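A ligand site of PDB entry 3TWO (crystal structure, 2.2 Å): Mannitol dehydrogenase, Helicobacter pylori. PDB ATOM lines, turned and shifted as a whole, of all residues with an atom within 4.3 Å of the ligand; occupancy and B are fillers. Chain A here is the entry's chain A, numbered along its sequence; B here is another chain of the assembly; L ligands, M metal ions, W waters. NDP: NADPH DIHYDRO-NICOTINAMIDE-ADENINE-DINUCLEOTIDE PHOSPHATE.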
ATOM      1  N   CYS A  42       2.817  -9.353 -22.697  1.00  0.00           N
ATOM      2  CA  CYS A  42       2.039 -10.220 -21.818  1.00  0.00           C
ATOM      3  C   CYS A  42       2.801 -11.523 -21.579  1.00  0.00           C
ATOM      4  O   CYS A  42       3.448 -12.043 -22.497  1.00  0.00           O
ATOM      5  CB  CYS A  42       0.714 -10.584 -22.487  1.00  0.00           C
ATOM      6  SG  CYS A  42      -0.408 -11.606 -21.421  1.00  0.00           S
ATOM      7  N   HIS A  43       2.710 -12.100 -20.375  1.00  0.00           N
ATOM      8  CA  HIS A  43       3.320 -13.422 -20.204  1.00  0.00           C
ATOM      9  C   HIS A  43       2.768 -14.477 -21.212  1.00  0.00           C
ATOM     10  O   HIS A  43       3.481 -15.449 -21.578  1.00  0.00           O
ATOM     11  CB  HIS A  43       3.184 -13.874 -18.756  1.00  0.00           C
ATOM     12  CG  HIS A  43       4.320 -14.736 -18.287  1.00  0.00           C
ATOM     13  ND1 HIS A  43       4.593 -15.969 -18.840  1.00  0.00           N
ATOM     14  CD2 HIS A  43       5.173 -14.591 -17.247  1.00  0.00           C
ATOM     15  CE1 HIS A  43       5.626 -16.503 -18.211  1.00  0.00           C
ATOM     16  NE2 HIS A  43       5.985 -15.699 -17.234  1.00  0.00           N
ATOM     17  N   SER A  44       1.511 -14.308 -21.685  1.00  0.00           N
ATOM     18  CA  SER A  44       1.007 -15.206 -22.734  1.00  0.00           C
ATOM     19  C   SER A  44       1.924 -15.164 -23.963  1.00  0.00           C
ATOM     20  O   SER A  44       2.074 -16.180 -24.649  1.00  0.00           O
ATOM     21  CB  SER A  44      -0.441 -14.857 -23.150  1.00  0.00           C
ATOM     22  OG  SER A  44      -1.336 -14.914 -22.012  1.00  0.00           O
ATOM     23  N   HIS A  47       4.685 -17.704 -23.149  1.00  0.00           N
ATOM     24  CA  HIS A  47       4.218 -19.087 -23.191  1.00  0.00           C
ATOM     25  C   HIS A  47       4.065 -19.561 -24.642  1.00  0.00           C
ATOM     26  O   HIS A  47       4.392 -20.695 -24.999  1.00  0.00           O
ATOM     27  CB  HIS A  47       2.843 -19.207 -22.516  1.00  0.00           C
ATOM     28  CG  HIS A  47       2.839 -18.959 -21.033  1.00  0.00           C
ATOM     29  ND1 HIS A  47       3.635 -19.657 -20.159  1.00  0.00           N
ATOM     30  CD2 HIS A  47       2.050 -18.146 -20.272  1.00  0.00           C
ATOM     31  CE1 HIS A  47       3.312 -19.327 -18.909  1.00  0.00           C
ATOM     32  NE2 HIS A  47       2.361 -18.400 -18.944  1.00  0.00           N
ATOM     33  N   TRP A  53       2.439 -24.208 -24.053  1.00  0.00           N
ATOM     34  CA  TRP A  53       1.060 -24.666 -24.031  1.00  0.00           C
ATOM     35  C   TRP A  53       0.753 -25.666 -25.137  1.00  0.00           C
ATOM     36  O   TRP A  53      -0.049 -26.547 -24.972  1.00  0.00           O
ATOM     37  CB  TRP A  53       0.110 -23.504 -24.227  1.00  0.00           C
ATOM     38  CG  TRP A  53       0.096 -22.431 -23.183  1.00  0.00           C
ATOM     39  CD1 TRP A  53       0.504 -22.518 -21.846  1.00  0.00           C
ATOM     40  CD2 TRP A  53      -0.398 -21.107 -23.369  1.00  0.00           C
ATOM     41  NE1 TRP A  53       0.303 -21.295 -21.228  1.00  0.00           N
ATOM     42  CE2 TRP A  53      -0.265 -20.432 -22.127  1.00  0.00           C
ATOM     43  CE3 TRP A  53      -0.941 -20.405 -24.477  1.00  0.00           C
ATOM     44  CZ2 TRP A  53      -0.660 -19.090 -21.964  1.00  0.00           C
ATOM     45  CZ3 TRP A  53      -1.314 -19.072 -24.319  1.00  0.00           C
ATOM     46  CH2 TRP A  53      -1.198 -18.439 -23.055  1.00  0.00           C
ATOM     47  N   CYS A 160      -5.385  -6.454 -22.811  1.00  0.00           N
ATOM     48  CA  CYS A 160      -5.427  -7.827 -22.389  1.00  0.00           C
ATOM     49  C   CYS A 160      -5.393  -7.949 -20.864  1.00  0.00           C
ATOM     50  O   CYS A 160      -6.275  -8.594 -20.308  1.00  0.00           O
ATOM     51  CB  CYS A 160      -4.312  -8.639 -23.007  1.00  0.00           C
ATOM     52  SG  CYS A 160      -4.453 -10.425 -22.380  1.00  0.00           S
ATOM     53  N   THR A 164      -8.996  -9.015 -18.844  1.00  0.00           N
ATOM     54  CA  THR A 164      -8.902 -10.347 -18.329  1.00  0.00           C
ATOM     55  C   THR A 164      -9.155 -10.361 -16.824  1.00  0.00           C
ATOM     56  O   THR A 164      -9.593 -11.394 -16.269  1.00  0.00           O
ATOM     57  CB  THR A 164      -7.496 -10.959 -18.657  1.00  0.00           C
ATOM     58  OG1 THR A 164      -7.325 -11.058 -20.095  1.00  0.00           O
ATOM     59  CG2 THR A 164      -7.338 -12.355 -17.974  1.00  0.00           C
ATOM     60  N   GLY A 184      -0.152 -13.733  -7.529  1.00  0.00           N
ATOM     61  CA  GLY A 184       0.750 -13.392  -8.616  1.00  0.00           C
ATOM     62  C   GLY A 184       0.579 -11.915  -8.906  1.00  0.00           C
ATOM     63  O   GLY A 184      -0.416 -11.494  -9.528  1.00  0.00           O
ATOM     64  N   PHE A 185       1.542 -11.124  -8.430  1.00  0.00           N
ATOM     65  CA  PHE A 185       1.479  -9.670  -8.478  1.00  0.00           C
ATOM     66  C   PHE A 185       2.303  -9.062  -9.644  1.00  0.00           C
ATOM     67  O   PHE A 185       3.244  -8.314  -9.444  1.00  0.00           O
ATOM     68  CB  PHE A 185       1.946  -9.133  -7.100  1.00  0.00           C
ATOM     69  CG  PHE A 185       1.752  -7.659  -6.906  1.00  0.00           C
ATOM     70  CD1 PHE A 185       0.608  -6.993  -7.402  1.00  0.00           C
ATOM     71  CD2 PHE A 185       2.694  -6.914  -6.199  1.00  0.00           C
ATOM     72  CE1 PHE A 185       0.423  -5.594  -7.187  1.00  0.00           C
ATOM     73  CE2 PHE A 185       2.506  -5.518  -5.952  1.00  0.00           C
ATOM     74  CZ  PHE A 185       1.380  -4.856  -6.440  1.00  0.00           C
ATOM     75  N   GLY A 186       1.898  -9.376 -10.863  1.00  0.00           N
ATOM     76  CA  GLY A 186       2.673  -9.033 -12.045  1.00  0.00           C
ATOM     77  C   GLY A 186       1.759  -8.168 -12.892  1.00  0.00           C
ATOM     78  O   GLY A 186       1.058  -7.301 -12.387  1.00  0.00           O
ATOM     79  N   GLY A 187       1.750  -8.390 -14.183  1.00  0.00           N
ATOM     80  CA  GLY A 187       0.956  -7.546 -15.042  1.00  0.00           C
ATOM     81  C   GLY A 187      -0.548  -7.651 -14.789  1.00  0.00           C
ATOM     82  O   GLY A 187      -1.187  -6.631 -14.591  1.00  0.00           O
ATOM     83  N   LEU A 188      -1.117  -8.861 -14.841  1.00  0.00           N
ATOM     84  CA  LEU A 188      -2.528  -9.001 -14.594  1.00  0.00           C
ATOM     85  C   LEU A 188      -2.773  -8.719 -13.091  1.00  0.00           C
ATOM     86  O   LEU A 188      -3.778  -8.115 -12.732  1.00  0.00           O
ATOM     87  CB  LEU A 188      -3.046 -10.417 -15.004  1.00  0.00           C
ATOM     88  CG  LEU A 188      -3.493 -10.663 -16.475  1.00  0.00           C
ATOM     89  CD1 LEU A 188      -2.307 -10.505 -17.494  1.00  0.00           C
ATOM     90  CD2 LEU A 188      -4.156 -12.073 -16.561  1.00  0.00           C
ATOM     91  N   PHE A 206      -0.833 -11.970  -2.977  1.00  0.00           N
ATOM     92  CA  PHE A 206      -0.013 -13.184  -2.698  1.00  0.00           C
ATOM     93  C   PHE A 206       1.112 -13.165  -3.744  1.00  0.00           C
ATOM     94  O   PHE A 206       0.863 -13.228  -4.951  1.00  0.00           O
ATOM     95  CB  PHE A 206      -0.851 -14.479  -2.806  1.00  0.00           C
ATOM     96  CG  PHE A 206      -1.989 -14.543  -1.808  1.00  0.00           C
ATOM     97  CD1 PHE A 206      -3.213 -13.905  -2.081  1.00  0.00           C
ATOM     98  CD2 PHE A 206      -1.801 -15.180  -0.592  1.00  0.00           C
ATOM     99  CE1 PHE A 206      -4.270 -13.894  -1.084  1.00  0.00           C
ATOM    100  CE2 PHE A 206      -2.836 -15.224   0.404  1.00  0.00           C
ATOM    101  CZ  PHE A 206      -4.086 -14.598   0.161  1.00  0.00           C
ATOM    102  N   ALA A 207       2.346 -13.045  -3.256  1.00  0.00           N
ATOM    103  CA  ALA A 207       3.529 -13.071  -4.081  1.00  0.00           C
ATOM    104  C   ALA A 207       4.488 -14.140  -3.546  1.00  0.00           C
ATOM    105  O   ALA A 207       4.194 -14.833  -2.556  1.00  0.00           O
ATOM    106  CB  ALA A 207       4.227 -11.692  -4.074  1.00  0.00           C
ATOM    107  N   ARG A 208       5.656 -14.213  -4.185  1.00  0.00           N
ATOM    108  CA  ARG A 208       6.728 -15.097  -3.732  1.00  0.00           C
ATOM    109  C   ARG A 208       7.771 -14.424  -2.819  1.00  0.00           C
ATOM    110  O   ARG A 208       8.518 -15.098  -2.170  1.00  0.00           O
ATOM    111  CB  ARG A 208       7.412 -15.737  -4.954  1.00  0.00           C
ATOM    112  CG  ARG A 208       6.421 -16.684  -5.697  1.00  0.00           C
ATOM    113  CD  ARG A 208       7.153 -17.607  -6.626  1.00  0.00           C
ATOM    114  NE  ARG A 208       7.602 -16.906  -7.846  1.00  0.00           N
ATOM    115  CZ  ARG A 208       8.118 -17.533  -8.906  1.00  0.00           C
ATOM    116  NH1 ARG A 208       8.255 -18.872  -8.905  1.00  0.00           N
ATOM    117  NH2 ARG A 208       8.516 -16.827  -9.959  1.00  0.00           N
ATOM    118  N   LYS A 212       8.037  -6.251  -3.930  1.00  0.00           N
ATOM    119  CA  LYS A 212       7.064  -5.226  -4.337  1.00  0.00           C
ATOM    120  C   LYS A 212       5.999  -4.901  -3.260  1.00  0.00           C
ATOM    121  O   LYS A 212       4.923  -4.351  -3.571  1.00  0.00           O
ATOM    122  CB  LYS A 212       6.452  -5.562  -5.711  1.00  0.00           C
ATOM    123  CG  LYS A 212       7.501  -5.638  -6.809  1.00  0.00           C
ATOM    124  CD  LYS A 212       6.957  -6.063  -8.211  1.00  0.00           C
ATOM    125  CE  LYS A 212       6.123  -7.324  -8.197  1.00  0.00           C
ATOM    126  NZ  LYS A 212       6.094  -7.892  -9.594  1.00  0.00           N
ATOM    127  N   THR A 241      -3.507 -15.311 -10.983  1.00  0.00           N
ATOM    128  CA  THR A 241      -2.769 -15.012 -12.235  1.00  0.00           C
ATOM    129  C   THR A 241      -1.458 -15.818 -12.334  1.00  0.00           C
ATOM    130  O   THR A 241      -0.653 -15.599 -13.235  1.00  0.00           O
ATOM    131  CB  THR A 241      -2.409 -13.527 -12.343  1.00  0.00           C
ATOM    132  OG1 THR A 241      -1.372 -13.213 -11.406  1.00  0.00           O
ATOM    133  CG2 THR A 241      -3.678 -12.643 -12.026  1.00  0.00           C
ATOM    134  N   ILE A 242      -1.260 -16.784 -11.440  1.00  0.00           N
ATOM    135  CA  ILE A 242       0.040 -17.470 -11.388  1.00  0.00           C
ATOM    136  C   ILE A 242       0.395 -18.233 -12.698  1.00  0.00           C
ATOM    137  O   ILE A 242      -0.395 -19.058 -13.189  1.00  0.00           O
ATOM    138  CB  ILE A 242       0.127 -18.387 -10.147  1.00  0.00           C
ATOM    139  CG1 ILE A 242       0.099 -17.544  -8.851  1.00  0.00           C
ATOM    140  CG2 ILE A 242       1.424 -19.225 -10.172  1.00  0.00           C
ATOM    141  CD1 ILE A 242      -0.283 -18.328  -7.622  1.00  0.00           C
ATOM    142  N   PRO A 243       1.588 -17.945 -13.293  1.00  0.00           N
ATOM    143  CA  PRO A 243       2.050 -18.625 -14.553  1.00  0.00           C
ATOM    144  C   PRO A 243       3.121 -19.719 -14.295  1.00  0.00           C
ATOM    145  O   PRO A 243       3.811 -20.116 -15.200  1.00  0.00           O
ATOM    146  CB  PRO A 243       2.662 -17.469 -15.354  1.00  0.00           C
ATOM    147  CG  PRO A 243       3.371 -16.656 -14.231  1.00  0.00           C
ATOM    148  CD  PRO A 243       2.475 -16.820 -12.949  1.00  0.00           C
ATOM    149  N   THR A 244       3.268 -20.164 -13.041  1.00  0.00           N
ATOM    150  CA  THR A 244       4.188 -21.237 -12.692  1.00  0.00           C
ATOM    151  C   THR A 244       3.411 -22.298 -11.894  1.00  0.00           C
ATOM    152  O   THR A 244       2.200 -22.108 -11.592  1.00  0.00           O
ATOM    153  CB  THR A 244       5.405 -20.758 -11.825  1.00  0.00           C
ATOM    154  OG1 THR A 244       4.950 -20.263 -10.568  1.00  0.00           O
ATOM    155  CG2 THR A 244       6.234 -19.649 -12.590  1.00  0.00           C
ATOM    156  N   HIS A 245       4.111 -23.384 -11.546  1.00  0.00           N
ATOM    157  CA  HIS A 245       3.423 -24.494 -10.892  1.00  0.00           C
ATOM    158  C   HIS A 245       3.024 -24.077  -9.511  1.00  0.00           C
ATOM    159  O   HIS A 245       3.773 -23.437  -8.844  1.00  0.00           O
ATOM    160  CB  HIS A 245       4.306 -25.748 -10.801  1.00  0.00           C
ATOM    161  CG  HIS A 245       3.596 -26.900 -10.199  1.00  0.00           C
ATOM    162  ND1 HIS A 245       3.921 -27.402  -8.956  1.00  0.00           N
ATOM    163  CD2 HIS A 245       2.543 -27.621 -10.629  1.00  0.00           C
ATOM    164  CE1 HIS A 245       3.100 -28.394  -8.659  1.00  0.00           C
ATOM    165  NE2 HIS A 245       2.258 -28.559  -9.654  1.00  0.00           N
ATOM    166  N   VAL A 264      -7.160 -17.416 -14.005  1.00  0.00           N
ATOM    167  CA  VAL A 264      -6.762 -16.862 -15.311  1.00  0.00           C
ATOM    168  C   VAL A 264      -5.355 -17.260 -15.726  1.00  0.00           C
ATOM    169  O   VAL A 264      -5.102 -17.441 -16.911  1.00  0.00           O
ATOM    170  CB  VAL A 264      -6.963 -15.316 -15.432  1.00  0.00           C
ATOM    171  CG1 VAL A 264      -8.470 -14.932 -15.247  1.00  0.00           C
ATOM    172  CG2 VAL A 264      -6.041 -14.518 -14.417  1.00  0.00           C
ATOM    173  N   GLY A 265      -4.465 -17.427 -14.751  1.00  0.00           N
ATOM    174  CA  GLY A 265      -3.053 -17.801 -15.024  1.00  0.00           C
ATOM    175  C   GLY A 265      -2.967 -19.169 -15.674  1.00  0.00           C
ATOM    176  O   GLY A 265      -3.770 -20.111 -15.370  1.00  0.00           O
ATOM    177  N   LEU A 266      -2.025 -19.300 -16.609  1.00  0.00           N
ATOM    178  CA  LEU A 266      -1.872 -20.517 -17.412  1.00  0.00           C
ATOM    179  C   LEU A 266      -0.409 -20.906 -17.454  1.00  0.00           C
ATOM    180  O   LEU A 266       0.322 -20.572 -18.412  1.00  0.00           O
ATOM    181  CB  LEU A 266      -2.319 -20.213 -18.842  1.00  0.00           C
ATOM    182  CG  LEU A 266      -3.652 -20.558 -19.506  1.00  0.00           C
ATOM    183  CD1 LEU A 266      -4.633 -21.410 -18.717  1.00  0.00           C
ATOM    184  CD2 LEU A 266      -4.295 -19.386 -20.181  1.00  0.00           C
ATOM    185  N   PRO A 267       0.058 -21.612 -16.407  1.00  0.00           N
ATOM    186  CA  PRO A 267       1.448 -22.144 -16.366  1.00  0.00           C
ATOM    187  C   PRO A 267       1.696 -23.105 -17.562  1.00  0.00           C
ATOM    188  O   PRO A 267       0.697 -23.585 -18.173  1.00  0.00           O
ATOM    189  CB  PRO A 267       1.478 -22.964 -15.066  1.00  0.00           C
ATOM    190  CG  PRO A 267       0.256 -22.570 -14.282  1.00  0.00           C
ATOM    191  CD  PRO A 267      -0.764 -22.019 -15.251  1.00  0.00           C
ATOM    192  N   SER A 291     -11.618 -17.930 -16.397  1.00  0.00           N
ATOM    193  CA  SER A 291     -12.084 -16.808 -17.222  1.00  0.00           C
ATOM    194  C   SER A 291     -11.083 -16.640 -18.347  1.00  0.00           C
ATOM    195  O   SER A 291      -9.843 -16.793 -18.136  1.00  0.00           O
ATOM    196  CB  SER A 291     -12.174 -15.541 -16.415  1.00  0.00           C
ATOM    197  OG  SER A 291     -12.908 -14.514 -17.075  1.00  0.00           O
ATOM    198  N   LEU A 292     -11.615 -16.469 -19.542  1.00  0.00           N
ATOM    199  CA  LEU A 292     -10.819 -16.226 -20.720  1.00  0.00           C
ATOM    200  C   LEU A 292     -11.036 -14.800 -21.289  1.00  0.00           C
ATOM    201  O   LEU A 292     -12.146 -14.522 -21.800  1.00  0.00           O
ATOM    202  CB  LEU A 292     -11.183 -17.246 -21.802  1.00  0.00           C
ATOM    203  CG  LEU A 292     -10.272 -17.244 -23.039  1.00  0.00           C
ATOM    204  CD1 LEU A 292      -8.800 -17.647 -22.799  1.00  0.00           C
ATOM    205  CD2 LEU A 292     -10.864 -18.168 -24.070  1.00  0.00           C
ATOM    206  N   ILE A 293      -9.969 -13.953 -21.225  1.00  0.00           N
ATOM    207  CA  ILE A 293      -9.992 -12.564 -21.778  1.00  0.00           C
ATOM    208  C   ILE A 293     -11.361 -11.957 -21.493  1.00  0.00           C
ATOM    209  O   ILE A 293     -11.812 -11.987 -20.359  1.00  0.00           O
ATOM    210  CB  ILE A 293      -9.850 -12.500 -23.338  1.00  0.00           C
ATOM    211  CG1 ILE A 293      -8.952 -13.597 -23.883  1.00  0.00           C
ATOM    212  CG2 ILE A 293      -9.189 -11.260 -23.737  1.00  0.00           C
ATOM    213  CD1 ILE A 293      -7.508 -13.442 -23.269  1.00  0.00           C
ATOM    214  N   LEU A 330      11.049 -11.542 -16.813  1.00  0.00           N
ATOM    215  CA  LEU A 330       9.746 -12.042 -16.501  1.00  0.00           C
ATOM    216  C   LEU A 330       9.783 -13.529 -16.149  1.00  0.00           C
ATOM    217  O   LEU A 330       8.832 -14.034 -15.507  1.00  0.00           O
ATOM    218  CB  LEU A 330       8.734 -11.793 -17.652  1.00  0.00           C
ATOM    219  CG  LEU A 330       8.211 -10.348 -17.813  1.00  0.00           C
ATOM    220  CD1 LEU A 330       7.741 -10.135 -19.233  1.00  0.00           C
ATOM    221  CD2 LEU A 330       7.115 -10.026 -16.800  1.00  0.00           C
ATOM    222  N   GLY A 333      12.104 -13.580 -12.244  1.00  0.00           N
ATOM    223  CA  GLY A 333      11.762 -12.840 -11.008  1.00  0.00           C
ATOM    224  C   GLY A 333      12.315 -11.428 -10.890  1.00  0.00           C
ATOM    225  O   GLY A 333      12.396 -10.878  -9.807  1.00  0.00           O
ATOM    226  N   PHE A 337       6.014  -4.603 -13.242  1.00  0.00           N
ATOM    227  CA  PHE A 337       4.628  -4.893 -13.625  1.00  0.00           C
ATOM    228  C   PHE A 337       4.556  -5.111 -15.120  1.00  0.00           C
ATOM    229  O   PHE A 337       4.932  -6.203 -15.554  1.00  0.00           O
ATOM    230  CB  PHE A 337       3.664  -3.841 -13.047  1.00  0.00           C
ATOM    231  CG  PHE A 337       3.739  -3.775 -11.555  1.00  0.00           C
ATOM    232  CD1 PHE A 337       4.385  -2.683 -10.913  1.00  0.00           C
ATOM    233  CD2 PHE A 337       3.311  -4.865 -10.770  1.00  0.00           C
ATOM    234  CE1 PHE A 337       4.535  -2.653  -9.495  1.00  0.00           C
ATOM    235  CE2 PHE A 337       3.432  -4.857  -9.375  1.00  0.00           C
ATOM    236  CZ  PHE A 337       4.060  -3.743  -8.732  1.00  0.00           C
ATOM    237  N   ARG A 338       4.197  -4.122 -15.926  1.00  0.00           N
ATOM    238  CA  ARG A 338       4.106  -4.375 -17.363  1.00  0.00           C
ATOM    239  C   ARG A 338       5.252  -3.722 -18.063  1.00  0.00           C
ATOM    240  O   ARG A 338       5.596  -2.603 -17.729  1.00  0.00           O
ATOM    241  CB  ARG A 338       2.801  -3.841 -17.966  1.00  0.00           C
ATOM    242  CG  ARG A 338       1.699  -4.865 -18.120  1.00  0.00           C
ATOM    243  CD  ARG A 338       2.070  -5.794 -19.279  1.00  0.00           C
ATOM    244  NE  ARG A 338       0.970  -6.650 -19.717  1.00  0.00           N
ATOM    245  CZ  ARG A 338       0.760  -7.886 -19.269  1.00  0.00           C
ATOM    246  NH1 ARG A 338       1.544  -8.452 -18.346  1.00  0.00           N
ATOM    247  NH2 ARG A 338      -0.253  -8.553 -19.776  1.00  0.00           N
ATOM    248  N   ILE B 281     -10.510 -22.610 -17.834  1.00  0.00           N
ATOM    249  CA  ILE B 281     -10.456 -21.427 -18.672  1.00  0.00           C
ATOM    250  C   ILE B 281     -11.098 -21.715 -20.028  1.00  0.00           C
ATOM    251  O   ILE B 281     -11.823 -20.857 -20.576  1.00  0.00           O
ATOM    252  CB  ILE B 281      -9.009 -20.903 -18.777  1.00  0.00           C
ATOM    253  CG1 ILE B 281      -8.677 -20.219 -17.425  1.00  0.00           C
ATOM    254  CG2 ILE B 281      -8.810 -19.923 -19.963  1.00  0.00           C
ATOM    255  CD1 ILE B 281      -7.217 -20.128 -17.115  1.00  0.00           C
HETATM  256  PA  NDP L   1       3.695 -11.641 -15.467  1.00  0.00           P
HETATM  257  O1A NDP L   1       4.904 -12.496 -15.269  1.00  0.00           O
HETATM  258  O2A NDP L   1       3.522 -10.122 -15.303  1.00  0.00           O
HETATM  259  O5B NDP L   1       3.241 -11.780 -13.931  1.00  0.00           O
HETATM  260  C5B NDP L   1       3.096 -13.027 -13.115  1.00  0.00           C
HETATM  261  C4B NDP L   1       3.315 -12.763 -11.638  1.00  0.00           C
HETATM  262  O4B NDP L   1       3.232 -14.005 -10.813  1.00  0.00           O
HETATM  263  C3B NDP L   1       4.803 -12.275 -11.443  1.00  0.00           C
HETATM  264  O3B NDP L   1       4.839 -11.089 -10.611  1.00  0.00           O
HETATM  265  C2B NDP L   1       5.502 -13.434 -10.677  1.00  0.00           C
HETATM  266  O2B NDP L   1       6.458 -12.893  -9.778  1.00  0.00           O
HETATM  267  C1B NDP L   1       4.352 -14.033  -9.850  1.00  0.00           C
HETATM  268  N9A NDP L   1       4.459 -15.445  -9.528  1.00  0.00           N
HETATM  269  C8A NDP L   1       5.020 -16.402 -10.314  1.00  0.00           C
HETATM  270  N7A NDP L   1       4.843 -17.573  -9.717  1.00  0.00           N
HETATM  271  C5A NDP L   1       4.161 -17.397  -8.582  1.00  0.00           C
HETATM  272  C6A NDP L   1       3.742 -18.255  -7.555  1.00  0.00           C
HETATM  273  N6A NDP L   1       3.949 -19.600  -7.570  1.00  0.00           N
HETATM  274  N1A NDP L   1       3.060 -17.730  -6.545  1.00  0.00           N
HETATM  275  C2A NDP L   1       2.827 -16.410  -6.445  1.00  0.00           C
HETATM  276  N3A NDP L   1       3.246 -15.573  -7.399  1.00  0.00           N
HETATM  277  C4A NDP L   1       3.901 -16.044  -8.481  1.00  0.00           C
HETATM  278  O3  NDP L   1       2.405 -12.430 -15.942  1.00  0.00           O
HETATM  279  PN  NDP L   1       1.082 -11.792 -16.557  1.00  0.00           P
HETATM  280  O1N NDP L   1       0.346 -11.033 -15.452  1.00  0.00           O
HETATM  281  O2N NDP L   1       1.282 -11.146 -17.954  1.00  0.00           O
HETATM  282  O5D NDP L   1       0.225 -13.092 -16.902  1.00  0.00           O
HETATM  283  C5D NDP L   1       0.202 -14.141 -15.874  1.00  0.00           C
HETATM  284  C4D NDP L   1      -0.493 -15.412 -16.425  1.00  0.00           C
HETATM  285  O4D NDP L   1      -1.783 -14.989 -16.902  1.00  0.00           O
HETATM  286  C3D NDP L   1       0.192 -16.064 -17.569  1.00  0.00           C
HETATM  287  O3D NDP L   1       0.077 -17.492 -17.416  1.00  0.00           O
HETATM  288  C2D NDP L   1      -0.627 -15.570 -18.751  1.00  0.00           C
HETATM  289  O2D NDP L   1      -0.545 -16.431 -19.888  1.00  0.00           O
HETATM  290  C1D NDP L   1      -2.028 -15.644 -18.153  1.00  0.00           C
HETATM  291  N1N NDP L   1      -3.025 -14.865 -18.946  1.00  0.00           N
HETATM  292  C2N NDP L   1      -4.308 -15.457 -19.075  1.00  0.00           C
HETATM  293  C3N NDP L   1      -5.288 -14.830 -19.794  1.00  0.00           C
HETATM  294  C7N NDP L   1      -6.689 -15.436 -19.855  1.00  0.00           C
HETATM  295  O7N NDP L   1      -7.081 -16.300 -19.042  1.00  0.00           O
HETATM  296  N7N NDP L   1      -7.492 -14.828 -20.675  1.00  0.00           N
HETATM  297  C4N NDP L   1      -4.984 -13.559 -20.383  1.00  0.00           C
HETATM  298  C5N NDP L   1      -3.721 -12.949 -20.220  1.00  0.00           C
HETATM  299  C6N NDP L   1      -2.710 -13.595 -19.507  1.00  0.00           C
HETATM  300  P2B NDP L   1       7.890 -13.517  -9.554  1.00  0.00           P
HETATM  301  O1X NDP L   1       8.854 -12.279  -9.777  1.00  0.00           O
HETATM  302  O2X NDP L   1       8.007 -14.206  -8.240  1.00  0.00           O
HETATM  303  O3X NDP L   1       8.123 -14.572 -10.760  1.00  0.00           O
HETATM  304 ZN    ZN M   1      -2.511 -11.572 -22.832  1.00  0.00          ZN
HETATM  305  O   HOH W   1       5.291  -8.466 -13.956  1.00  0.00           O
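The side-chain amino group of Lys 212 is in hydrogen-bond range of the backbone carbonyl oxygen of Phe 185 (2.9 Å).
A ring nitrogen (ND1) of His 43 lies within hydrogen-bond range of a ring nitrogen (NE2) of His 47 (3.3 Å).
O of Leu 266 sits at hydrogen-bond distance from NE1 of Trp 53, at 2.9 Å.
NH2 of Arg 338 sits close to SG of Cys 42, at 3.5 Å.
SG of Cys 42 lies close to N of Ser 44.
O of Cys 160 is in hydrogen-bond range of OG1 of Thr 164 (2.7 Å).
The backbone carbonyl oxygen (O) of Phe 206 is in hydrogen-bond range of the backbone NH (N) of Gly 184, 2.8 Å away.
The backbone carbonyl oxygen of Leu 266 is in hydrogen-bond range of a ring nitrogen (NE2) of His 47.
NE2 of His 47 sits at hydrogen-bond distance from O3D of the ligand, at 2.9 Å.
The backbone NH (N) of His 43 is in hydrogen-bond range of an oxygen (O2N) of the ligand (3.0 Å).
O2D of the ligand lies within hydrogen-bond range of OG of Ser 44.
An oxygen (O2A) of the ligand sits at hydrogen-bond distance from the backbone NH (N) of Gly 187 (2.7 Å).
The backbone NH of Ile 293 lies close to a nitrogen (N7N) of the ligand (2.7 Å).
The guanidinium group of Arg 338 lies within salt-bridge range of an oxygen (O2N) of the ligand (2.7 Å).
NH2 of Arg 208 is in salt-bridge range of O3X of the ligand (2.4 Å).
The backbone carbonyl oxygen (O) of Leu 266 lies within hydrogen-bond range of an oxygen (O3D) of the ligand (3.2 Å).
The side-chain hydroxyl of Thr 244 lies within hydrogen-bond range of a nitrogen (N7A) of the ligand, 2.8 Å away.
The backbone NH of Leu 266 sits at hydrogen-bond distance from an oxygen (O3D) of the ligand (2.9 Å).
An oxygen (O3B) of the ligand lies close to the backbone NH of Gly 186 (3.4 Å).
N of Leu 188 lies within hydrogen-bond range of O1N of the ligand, 2.7 Å away.
The backbone NH of Ser 44 is in hydrogen-bond range of an oxygen (O2D) of the ligand (3.5 Å).
O3B of the ligand sits close to O of Phe 185, at 3.4 Å.
Water W1 bridges O2A of the ligand and O of Phe 337.
The backbone carbonyl oxygen (O) of Val 264 lies close to an oxygen (O7N) of the ligand, at 3.1 Å.
The backbone carbonyl oxygen (O) of Ser 291 sits close to an oxygen (O7N) of the ligand.
Merely in contact with the ligand: Cys 42 (3.6 Å), Trp 53 (3.4 Å), Cys 160 (3.4 Å), Thr 164 (3.4 Å), Gly 184 (3.4 Å), Lys 212 (3.6 Å), Thr 241 (3.1 Å), Ile 242 (3.6 Å), Pro 243 (3.3 Å), Gly 265 (3.6 Å), Leu 292 (3.6 Å), Leu 330 (3.7 Å) and Gly 333 (3.2 Å).
Within 4 Å of the ligand: Cys 42, His 43, Ser 44, His 47, Trp 53, Cys 160, Thr 164, Gly 184, Phe 185, Gly 186, Gly 187, Leu 188, Arg 208, Lys 212, Thr 241, Ile 242, Pro 243, Thr 244, Val 264, Gly 265, Leu 266, Ser 291, Leu 292, Ile 293, Leu 330, Gly 333 and Arg 338.
The nearest printed residue that does not touch the ligand is Phe 206 (4.03 Å).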
